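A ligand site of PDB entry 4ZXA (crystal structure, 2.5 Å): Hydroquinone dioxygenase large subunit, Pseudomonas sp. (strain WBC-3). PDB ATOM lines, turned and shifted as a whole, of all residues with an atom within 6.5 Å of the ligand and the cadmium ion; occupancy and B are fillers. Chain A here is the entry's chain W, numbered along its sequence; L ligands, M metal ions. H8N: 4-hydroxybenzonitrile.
An oxygen (OAB) of the ligand lies within hydrogen-bond range of the side-chain carboxylate of Glu 248, at 2.4 Å.
The side-chain amide nitrogen (ND2) of Asn 258 sits at hydrogen-bond distance from the backbone carbonyl oxygen (O) of Met 297 (3.4 Å).
N of Asn 258 sits at hydrogen-bond distance from O of Ile 301 (3.0 Å).
O of Glu 262 lies within hydrogen-bond range of N of Met 297 (2.6 Å).
N of Trp 230 lies within hydrogen-bond range of OE1 of Glu 248 (3.0 Å).
N of Asn 231 lies within hydrogen-bond range of OG1 of Thr 246.
O of Leu 313 lies within hydrogen-bond range of N of Thr 246 (2.9 Å).
N of Trp 230 sits at hydrogen-bond distance from O of Thr 247, at 3.2 Å.
NE1 of Trp 76 sits at hydrogen-bond distance from OD1 of Asn 231 (3.0 Å).
Residues that only touch the ligand: Thr 246 (3.3 Å), Trp 230 (3.4 Å), Pro 232 (3.5 Å), Trp 273 (3.6 Å), Phe 79 (3.7 Å), Asn 231 (3.7 Å), Phe 264 (3.7 Å), Trp 76 (3.8 Å) and Leu 252 (3.9 Å).
13 residues have an atom within 4 Å of the ligand: Trp 76, Phe 79, Trp 230, Asn 231, Pro 232, Thr 246, Glu 248, Leu 252, His 256, Glu 262, Phe 264, Trp 273 and His 303.
The nearest printed residue that does not touch the ligand is Leu 313 (4.1 Å).
Of the 23 residues printed, 4 come within 4 Å of the cadmium ion.
The nearest printed residue that does not touch the cadmium ion is Phe 79 (4.8 Å).
The cadmium ion is bound by a ring nitrogen (ND1) of His 256 (2.2 Å), a ring nitrogen (NE2) of His 303 (2.2 Å), the side-chain amide oxygen (OD1) of Asn 258 (2.3 Å), a nitrogen (NAA) of the ligand (2.3 Å), the side-chain carboxylate (OE1) of Glu 262 (2.4 Å) and the side-chain carboxylate (OE2) of Glu 262 (2.5 Å).
The cadmium ion has six donor atoms within binding distance.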
ATOM      1  N   TRP A  76     -20.167  -5.621  36.505  1.00  0.00           N
ATOM      2  CA  TRP A  76     -20.286  -7.078  36.569  1.00  0.00           C
ATOM      3  C   TRP A  76     -19.604  -7.655  37.806  1.00  0.00           C
ATOM      4  O   TRP A  76     -19.626  -8.861  38.024  1.00  0.00           O
ATOM      5  CB  TRP A  76     -19.679  -7.744  35.329  1.00  0.00           C
ATOM      6  CG  TRP A  76     -20.285  -7.314  34.032  1.00  0.00           C
ATOM      7  CD1 TRP A  76     -21.455  -6.620  33.861  1.00  0.00           C
ATOM      8  CD2 TRP A  76     -19.747  -7.531  32.721  1.00  0.00           C
ATOM      9  NE1 TRP A  76     -21.675  -6.404  32.524  1.00  0.00           N
ATOM     10  CE2 TRP A  76     -20.642  -6.945  31.798  1.00  0.00           C
ATOM     11  CE3 TRP A  76     -18.600  -8.155  32.231  1.00  0.00           C
ATOM     12  CZ2 TRP A  76     -20.429  -6.982  30.433  1.00  0.00           C
ATOM     13  CZ3 TRP A  76     -18.382  -8.188  30.882  1.00  0.00           C
ATOM     14  CH2 TRP A  76     -19.288  -7.600  29.986  1.00  0.00           C
ATOM     15  N   PHE A  79     -17.081 -10.186  36.952  1.00  0.00           N
ATOM     16  CA  PHE A  79     -17.586 -11.277  36.141  1.00  0.00           C
ATOM     17  C   PHE A  79     -16.986 -12.613  36.589  1.00  0.00           C
ATOM     18  O   PHE A  79     -16.859 -12.875  37.785  1.00  0.00           O
ATOM     19  CB  PHE A  79     -17.260 -10.997  34.674  1.00  0.00           C
ATOM     20  CG  PHE A  79     -18.246 -11.596  33.703  1.00  0.00           C
ATOM     21  CD1 PHE A  79     -19.500 -12.004  34.125  1.00  0.00           C
ATOM     22  CD2 PHE A  79     -17.907 -11.757  32.369  1.00  0.00           C
ATOM     23  CE1 PHE A  79     -20.410 -12.570  33.230  1.00  0.00           C
ATOM     24  CE2 PHE A  79     -18.803 -12.323  31.464  1.00  0.00           C
ATOM     25  CZ  PHE A  79     -20.061 -12.724  31.892  1.00  0.00           C
ATOM     26  N   THR A 229     -26.085  -1.185  27.192  1.00  0.00           N
ATOM     27  CA  THR A 229     -25.736  -2.292  26.321  1.00  0.00           C
ATOM     28  C   THR A 229     -24.755  -3.268  26.962  1.00  0.00           C
ATOM     29  O   THR A 229     -24.026  -2.921  27.872  1.00  0.00           O
ATOM     30  CB  THR A 229     -25.144  -1.796  25.004  1.00  0.00           C
ATOM     31  OG1 THR A 229     -23.909  -1.127  25.274  1.00  0.00           O
ATOM     32  CG2 THR A 229     -26.097  -0.848  24.330  1.00  0.00           C
ATOM     33  N   TRP A 230     -24.749  -4.497  26.462  1.00  0.00           N
ATOM     34  CA  TRP A 230     -23.883  -5.543  26.979  1.00  0.00           C
ATOM     35  C   TRP A 230     -23.901  -5.599  28.504  1.00  0.00           C
ATOM     36  O   TRP A 230     -22.871  -5.423  29.174  1.00  0.00           O
ATOM     37  CB  TRP A 230     -22.484  -5.366  26.440  1.00  0.00           C
ATOM     38  CG  TRP A 230     -22.459  -5.231  24.940  1.00  0.00           C
ATOM     39  CD1 TRP A 230     -22.410  -4.081  24.225  1.00  0.00           C
ATOM     40  CD2 TRP A 230     -22.501  -6.304  23.989  1.00  0.00           C
ATOM     41  NE1 TRP A 230     -22.408  -4.355  22.881  1.00  0.00           N
ATOM     42  CE2 TRP A 230     -22.461  -5.712  22.710  1.00  0.00           C
ATOM     43  CE3 TRP A 230     -22.561  -7.694  24.089  1.00  0.00           C
ATOM     44  CZ2 TRP A 230     -22.467  -6.479  21.534  1.00  0.00           C
ATOM     45  CZ3 TRP A 230     -22.566  -8.450  22.935  1.00  0.00           C
ATOM     46  CH2 TRP A 230     -22.514  -7.839  21.674  1.00  0.00           C
ATOM     47  N   ASN A 231     -25.105  -5.829  29.041  1.00  0.00           N
ATOM     48  CA  ASN A 231     -25.280  -5.920  30.476  1.00  0.00           C
ATOM     49  C   ASN A 231     -26.341  -6.922  30.921  1.00  0.00           C
ATOM     50  O   ASN A 231     -27.478  -6.553  31.203  1.00  0.00           O
ATOM     51  CB  ASN A 231     -25.565  -4.546  31.068  1.00  0.00           C
ATOM     52  CG  ASN A 231     -25.304  -4.493  32.554  1.00  0.00           C
ATOM     53  OD1 ASN A 231     -24.246  -4.907  33.030  1.00  0.00           O
ATOM     54  ND2 ASN A 231     -26.273  -4.001  33.314  1.00  0.00           N
ATOM     55  N   PRO A 232     -25.962  -8.195  30.985  1.00  0.00           N
ATOM     56  CA  PRO A 232     -26.880  -9.245  31.423  1.00  0.00           C
ATOM     57  C   PRO A 232     -27.511  -8.852  32.761  1.00  0.00           C
ATOM     58  O   PRO A 232     -26.792  -8.565  33.711  1.00  0.00           O
ATOM     59  CB  PRO A 232     -25.978 -10.473  31.599  1.00  0.00           C
ATOM     60  CG  PRO A 232     -24.799 -10.201  30.652  1.00  0.00           C
ATOM     61  CD  PRO A 232     -24.599  -8.714  30.742  1.00  0.00           C
ATOM     62  N   THR A 246     -30.203  -9.149  27.915  1.00  0.00           N
ATOM     63  CA  THR A 246     -29.513  -7.880  27.753  1.00  0.00           C
ATOM     64  C   THR A 246     -29.623  -7.452  26.293  1.00  0.00           C
ATOM     65  O   THR A 246     -29.808  -8.285  25.413  1.00  0.00           O
ATOM     66  CB  THR A 246     -28.022  -8.009  28.160  1.00  0.00           C
ATOM     67  OG1 THR A 246     -27.332  -6.789  27.868  1.00  0.00           O
ATOM     68  CG2 THR A 246     -27.365  -9.144  27.416  1.00  0.00           C
ATOM     69  N   THR A 247     -29.544  -6.148  26.033  1.00  0.00           N
ATOM     70  CA  THR A 247     -29.642  -5.612  24.689  1.00  0.00           C
ATOM     71  C   THR A 247     -28.254  -5.226  24.203  1.00  0.00           C
ATOM     72  O   THR A 247     -27.568  -4.447  24.850  1.00  0.00           O
ATOM     73  CB  THR A 247     -30.619  -4.416  24.631  1.00  0.00           C
ATOM     74  OG1 THR A 247     -30.096  -3.336  25.398  1.00  0.00           O
ATOM     75  CG2 THR A 247     -31.978  -4.834  25.213  1.00  0.00           C
ATOM     76  N   GLU A 248     -27.845  -5.782  23.064  1.00  0.00           N
ATOM     77  CA  GLU A 248     -26.486  -5.654  22.583  1.00  0.00           C
ATOM     78  C   GLU A 248     -26.410  -4.814  21.318  1.00  0.00           C
ATOM     79  O   GLU A 248     -27.153  -5.020  20.353  1.00  0.00           O
ATOM     80  CB  GLU A 248     -25.885  -7.039  22.314  1.00  0.00           C
ATOM     81  CG  GLU A 248     -26.399  -8.153  23.201  1.00  0.00           C
ATOM     82  CD  GLU A 248     -25.935  -8.047  24.656  1.00  0.00           C
ATOM     83  OE1 GLU A 248     -26.021  -6.947  25.259  1.00  0.00           O
ATOM     84  OE2 GLU A 248     -25.489  -9.083  25.197  1.00  0.00           O
ATOM     85  N   LEU A 252     -19.114  -5.979  21.970  1.00  0.00           N
ATOM     86  CA  LEU A 252     -18.848  -6.308  23.379  1.00  0.00           C
ATOM     87  C   LEU A 252     -17.581  -5.570  23.827  1.00  0.00           C
ATOM     88  O   LEU A 252     -16.509  -5.754  23.258  1.00  0.00           O
ATOM     89  CB  LEU A 252     -18.675  -7.827  23.550  1.00  0.00           C
ATOM     90  CG  LEU A 252     -18.407  -8.327  24.974  1.00  0.00           C
ATOM     91  CD1 LEU A 252     -19.588  -8.050  25.903  1.00  0.00           C
ATOM     92  CD2 LEU A 252     -18.045  -9.816  24.976  1.00  0.00           C
ATOM     93  N   VAL A 254     -15.331  -5.893  25.850  1.00  0.00           N
ATOM     94  CA  VAL A 254     -14.174  -6.666  26.242  1.00  0.00           C
ATOM     95  C   VAL A 254     -14.184  -7.931  25.424  1.00  0.00           C
ATOM     96  O   VAL A 254     -15.204  -8.264  24.861  1.00  0.00           O
ATOM     97  CB  VAL A 254     -14.237  -7.098  27.739  1.00  0.00           C
ATOM     98  CG1 VAL A 254     -14.134  -5.897  28.648  1.00  0.00           C
ATOM     99  CG2 VAL A 254     -15.509  -7.899  28.032  1.00  0.00           C
ATOM    100  N   HIS A 256     -13.898 -11.908  26.302  1.00  0.00           N
ATOM    101  CA  HIS A 256     -14.040 -12.680  27.522  1.00  0.00           C
ATOM    102  C   HIS A 256     -13.386 -14.047  27.406  1.00  0.00           C
ATOM    103  O   HIS A 256     -13.635 -14.773  26.449  1.00  0.00           O
ATOM    104  CB  HIS A 256     -15.521 -12.865  27.860  1.00  0.00           C
ATOM    105  CG  HIS A 256     -15.740 -13.528  29.172  1.00  0.00           C
ATOM    106  ND1 HIS A 256     -16.784 -14.391  29.407  1.00  0.00           N
ATOM    107  CD2 HIS A 256     -15.045 -13.470  30.322  1.00  0.00           C
ATOM    108  CE1 HIS A 256     -16.738 -14.829  30.642  1.00  0.00           C
ATOM    109  NE2 HIS A 256     -15.688 -14.284  31.227  1.00  0.00           N
ATOM    110  N   GLY A 257     -12.554 -14.383  28.382  1.00  0.00           N
ATOM    111  CA  GLY A 257     -12.016 -15.728  28.501  1.00  0.00           C
ATOM    112  C   GLY A 257     -12.811 -16.515  29.524  1.00  0.00           C
ATOM    113  O   GLY A 257     -12.857 -16.136  30.700  1.00  0.00           O
ATOM    114  N   ASN A 258     -13.466 -17.585  29.086  1.00  0.00           N
ATOM    115  CA  ASN A 258     -14.409 -18.334  29.911  1.00  0.00           C
ATOM    116  C   ASN A 258     -13.784 -19.194  31.025  1.00  0.00           C
ATOM    117  O   ASN A 258     -12.632 -19.593  30.916  1.00  0.00           O
ATOM    118  CB  ASN A 258     -15.288 -19.216  29.009  1.00  0.00           C
ATOM    119  CG  ASN A 258     -16.436 -18.451  28.365  1.00  0.00           C
ATOM    120  OD1 ASN A 258     -16.441 -17.218  28.309  1.00  0.00           O
ATOM    121  ND2 ASN A 258     -17.427 -19.197  27.872  1.00  0.00           N
ATOM    122  N   ARG A 260     -16.377 -21.356  32.732  1.00  0.00           N
ATOM    123  CA  ARG A 260     -17.517 -22.236  32.874  1.00  0.00           C
ATOM    124  C   ARG A 260     -18.201 -22.228  31.520  1.00  0.00           C
ATOM    125  O   ARG A 260     -17.916 -21.362  30.710  1.00  0.00           O
ATOM    126  CB  ARG A 260     -18.475 -21.717  33.943  1.00  0.00           C
ATOM    127  CG  ARG A 260     -18.922 -20.280  33.743  1.00  0.00           C
ATOM    128  CD  ARG A 260     -19.403 -19.640  35.045  1.00  0.00           C
ATOM    129  NE  ARG A 260     -18.294 -19.596  35.995  1.00  0.00           N
ATOM    130  CZ  ARG A 260     -18.425 -19.529  37.320  1.00  0.00           C
ATOM    131  NH1 ARG A 260     -19.629 -19.482  37.862  1.00  0.00           N
ATOM    132  NH2 ARG A 260     -17.327 -19.494  38.079  1.00  0.00           N
ATOM    133  N   GLU A 262     -21.113 -21.274  29.074  1.00  0.00           N
ATOM    134  CA  GLU A 262     -22.188 -20.282  29.030  1.00  0.00           C
ATOM    135  C   GLU A 262     -23.208 -20.666  27.983  1.00  0.00           C
ATOM    136  O   GLU A 262     -22.851 -21.324  27.000  1.00  0.00           O
ATOM    137  CB  GLU A 262     -21.631 -18.911  28.647  1.00  0.00           C
ATOM    138  CG  GLU A 262     -20.716 -18.317  29.669  1.00  0.00           C
ATOM    139  CD  GLU A 262     -19.847 -17.225  29.089  1.00  0.00           C
ATOM    140  OE1 GLU A 262     -19.702 -17.183  27.843  1.00  0.00           O
ATOM    141  OE2 GLU A 262     -19.313 -16.408  29.875  1.00  0.00           O
ATOM    142  N   PHE A 264     -26.146 -19.017  25.361  1.00  0.00           N
ATOM    143  CA  PHE A 264     -26.725 -17.853  24.710  1.00  0.00           C
ATOM    144  C   PHE A 264     -27.980 -18.285  23.915  1.00  0.00           C
ATOM    145  O   PHE A 264     -27.919 -19.216  23.108  1.00  0.00           O
ATOM    146  CB  PHE A 264     -25.709 -17.251  23.736  1.00  0.00           C
ATOM    147  CG  PHE A 264     -24.508 -16.618  24.389  1.00  0.00           C
ATOM    148  CD1 PHE A 264     -24.484 -16.323  25.740  1.00  0.00           C
ATOM    149  CD2 PHE A 264     -23.380 -16.298  23.629  1.00  0.00           C
ATOM    150  CE1 PHE A 264     -23.365 -15.734  26.345  1.00  0.00           C
ATOM    151  CE2 PHE A 264     -22.256 -15.710  24.221  1.00  0.00           C
ATOM    152  CZ  PHE A 264     -22.252 -15.425  25.574  1.00  0.00           C
ATOM    153  N   TRP A 273     -20.184 -13.945  16.883  1.00  0.00           N
ATOM    154  CA  TRP A 273     -19.148 -14.243  17.868  1.00  0.00           C
ATOM    155  C   TRP A 273     -17.854 -14.771  17.256  1.00  0.00           C
ATOM    156  O   TRP A 273     -17.862 -15.786  16.552  1.00  0.00           O
ATOM    157  CB  TRP A 273     -19.685 -15.212  18.922  1.00  0.00           C
ATOM    158  CG  TRP A 273     -20.741 -14.618  19.777  1.00  0.00           C
ATOM    159  CD1 TRP A 273     -22.090 -14.642  19.538  1.00  0.00           C
ATOM    160  CD2 TRP A 273     -20.570 -13.888  20.999  1.00  0.00           C
ATOM    161  NE1 TRP A 273     -22.757 -13.992  20.548  1.00  0.00           N
ATOM    162  CE2 TRP A 273     -21.851 -13.513  21.449  1.00  0.00           C
ATOM    163  CE3 TRP A 273     -19.450 -13.522  21.760  1.00  0.00           C
ATOM    164  CZ2 TRP A 273     -22.051 -12.797  22.632  1.00  0.00           C
ATOM    165  CZ3 TRP A 273     -19.650 -12.800  22.935  1.00  0.00           C
ATOM    166  CH2 TRP A 273     -20.937 -12.445  23.354  1.00  0.00           C
ATOM    167  N   MET A 297     -21.383 -21.723  24.866  1.00  0.00           N
ATOM    168  CA  MET A 297     -20.002 -21.289  24.758  1.00  0.00           C
ATOM    169  C   MET A 297     -19.139 -22.056  25.775  1.00  0.00           C
ATOM    170  O   MET A 297     -19.315 -21.912  26.987  1.00  0.00           O
ATOM    171  CB  MET A 297     -19.916 -19.764  24.940  1.00  0.00           C
ATOM    172  CG  MET A 297     -20.631 -18.961  23.844  1.00  0.00           C
ATOM    173  SD  MET A 297     -19.700 -18.941  22.289  1.00  0.00           S
ATOM    174  CE  MET A 297     -20.874 -18.159  21.161  1.00  0.00           C
ATOM    175  N   ILE A 301     -12.677 -21.494  25.862  1.00  0.00           N
ATOM    176  CA  ILE A 301     -12.468 -20.553  24.778  1.00  0.00           C
ATOM    177  C   ILE A 301     -12.568 -19.134  25.303  1.00  0.00           C
ATOM    178  O   ILE A 301     -12.937 -18.897  26.446  1.00  0.00           O
ATOM    179  CB  ILE A 301     -13.469 -20.797  23.575  1.00  0.00           C
ATOM    180  CG1 ILE A 301     -14.929 -20.843  24.043  1.00  0.00           C
ATOM    181  CG2 ILE A 301     -13.131 -22.083  22.828  1.00  0.00           C
ATOM    182  CD1 ILE A 301     -15.536 -19.495  24.358  1.00  0.00           C
ATOM    183  N   HIS A 303     -13.979 -15.189  23.612  1.00  0.00           N
ATOM    184  CA  HIS A 303     -14.857 -14.752  22.543  1.00  0.00           C
ATOM    185  C   HIS A 303     -15.249 -13.291  22.683  1.00  0.00           C
ATOM    186  O   HIS A 303     -15.043 -12.696  23.734  1.00  0.00           O
ATOM    187  CB  HIS A 303     -16.103 -15.650  22.499  1.00  0.00           C
ATOM    188  CG  HIS A 303     -16.866 -15.681  23.783  1.00  0.00           C
ATOM    189  ND1 HIS A 303     -17.952 -16.493  23.976  1.00  0.00           N
ATOM    190  CD2 HIS A 303     -16.693 -14.984  24.926  1.00  0.00           C
ATOM    191  CE1 HIS A 303     -18.433 -16.301  25.196  1.00  0.00           C
ATOM    192  NE2 HIS A 303     -17.686 -15.388  25.792  1.00  0.00           N
ATOM    193  N   LEU A 313     -30.677 -10.380  23.531  1.00  0.00           N
ATOM    194  CA  LEU A 313     -29.950 -11.620  23.790  1.00  0.00           C
ATOM    195  C   LEU A 313     -30.268 -12.144  25.175  1.00  0.00           C
ATOM    196  O   LEU A 313     -30.238 -11.395  26.158  1.00  0.00           O
ATOM    197  CB  LEU A 313     -28.427 -11.427  23.647  1.00  0.00           C
ATOM    198  CG  LEU A 313     -27.550 -12.588  24.147  1.00  0.00           C
ATOM    199  CD1 LEU A 313     -27.747 -13.834  23.292  1.00  0.00           C
ATOM    200  CD2 LEU A 313     -26.095 -12.218  24.152  1.00  0.00           C
ATOM    201  N   VAL A 315     -28.876 -14.295  28.087  1.00  0.00           N
ATOM    202  CA  VAL A 315     -27.740 -14.996  28.691  1.00  0.00           C
ATOM    203  C   VAL A 315     -28.252 -15.832  29.870  1.00  0.00           C
ATOM    204  O   VAL A 315     -28.838 -15.315  30.822  1.00  0.00           O
ATOM    205  CB  VAL A 315     -26.625 -14.025  29.178  1.00  0.00           C
ATOM    206  CG1 VAL A 315     -25.445 -14.825  29.746  1.00  0.00           C
ATOM    207  CG2 VAL A 315     -26.183 -13.099  28.049  1.00  0.00           C
HETATM  208  NAA H8N L   1     -19.273 -13.548  28.037  1.00  0.00           N
HETATM  209  CAC H8N L   1     -20.069 -12.734  27.926  1.00  0.00           C
HETATM  210  CAI H8N L   1     -21.131 -11.702  27.748  1.00  0.00           C
HETATM  211  CAF H8N L   1     -22.058 -11.876  26.731  1.00  0.00           C
HETATM  212  CAD H8N L   1     -23.060 -10.931  26.529  1.00  0.00           C
HETATM  213  CAH H8N L   1     -23.097  -9.830  27.375  1.00  0.00           C
HETATM  214  OAB H8N L   1     -24.077  -8.895  27.181  1.00  0.00           O
HETATM  215  CAE H8N L   1     -22.171  -9.662  28.400  1.00  0.00           C
HETATM  216  CAG H8N L   1     -21.177 -10.603  28.591  1.00  0.00           C
HETATM  217 CD    CD M   1     -17.997 -15.506  27.980  1.00  0.00          CD
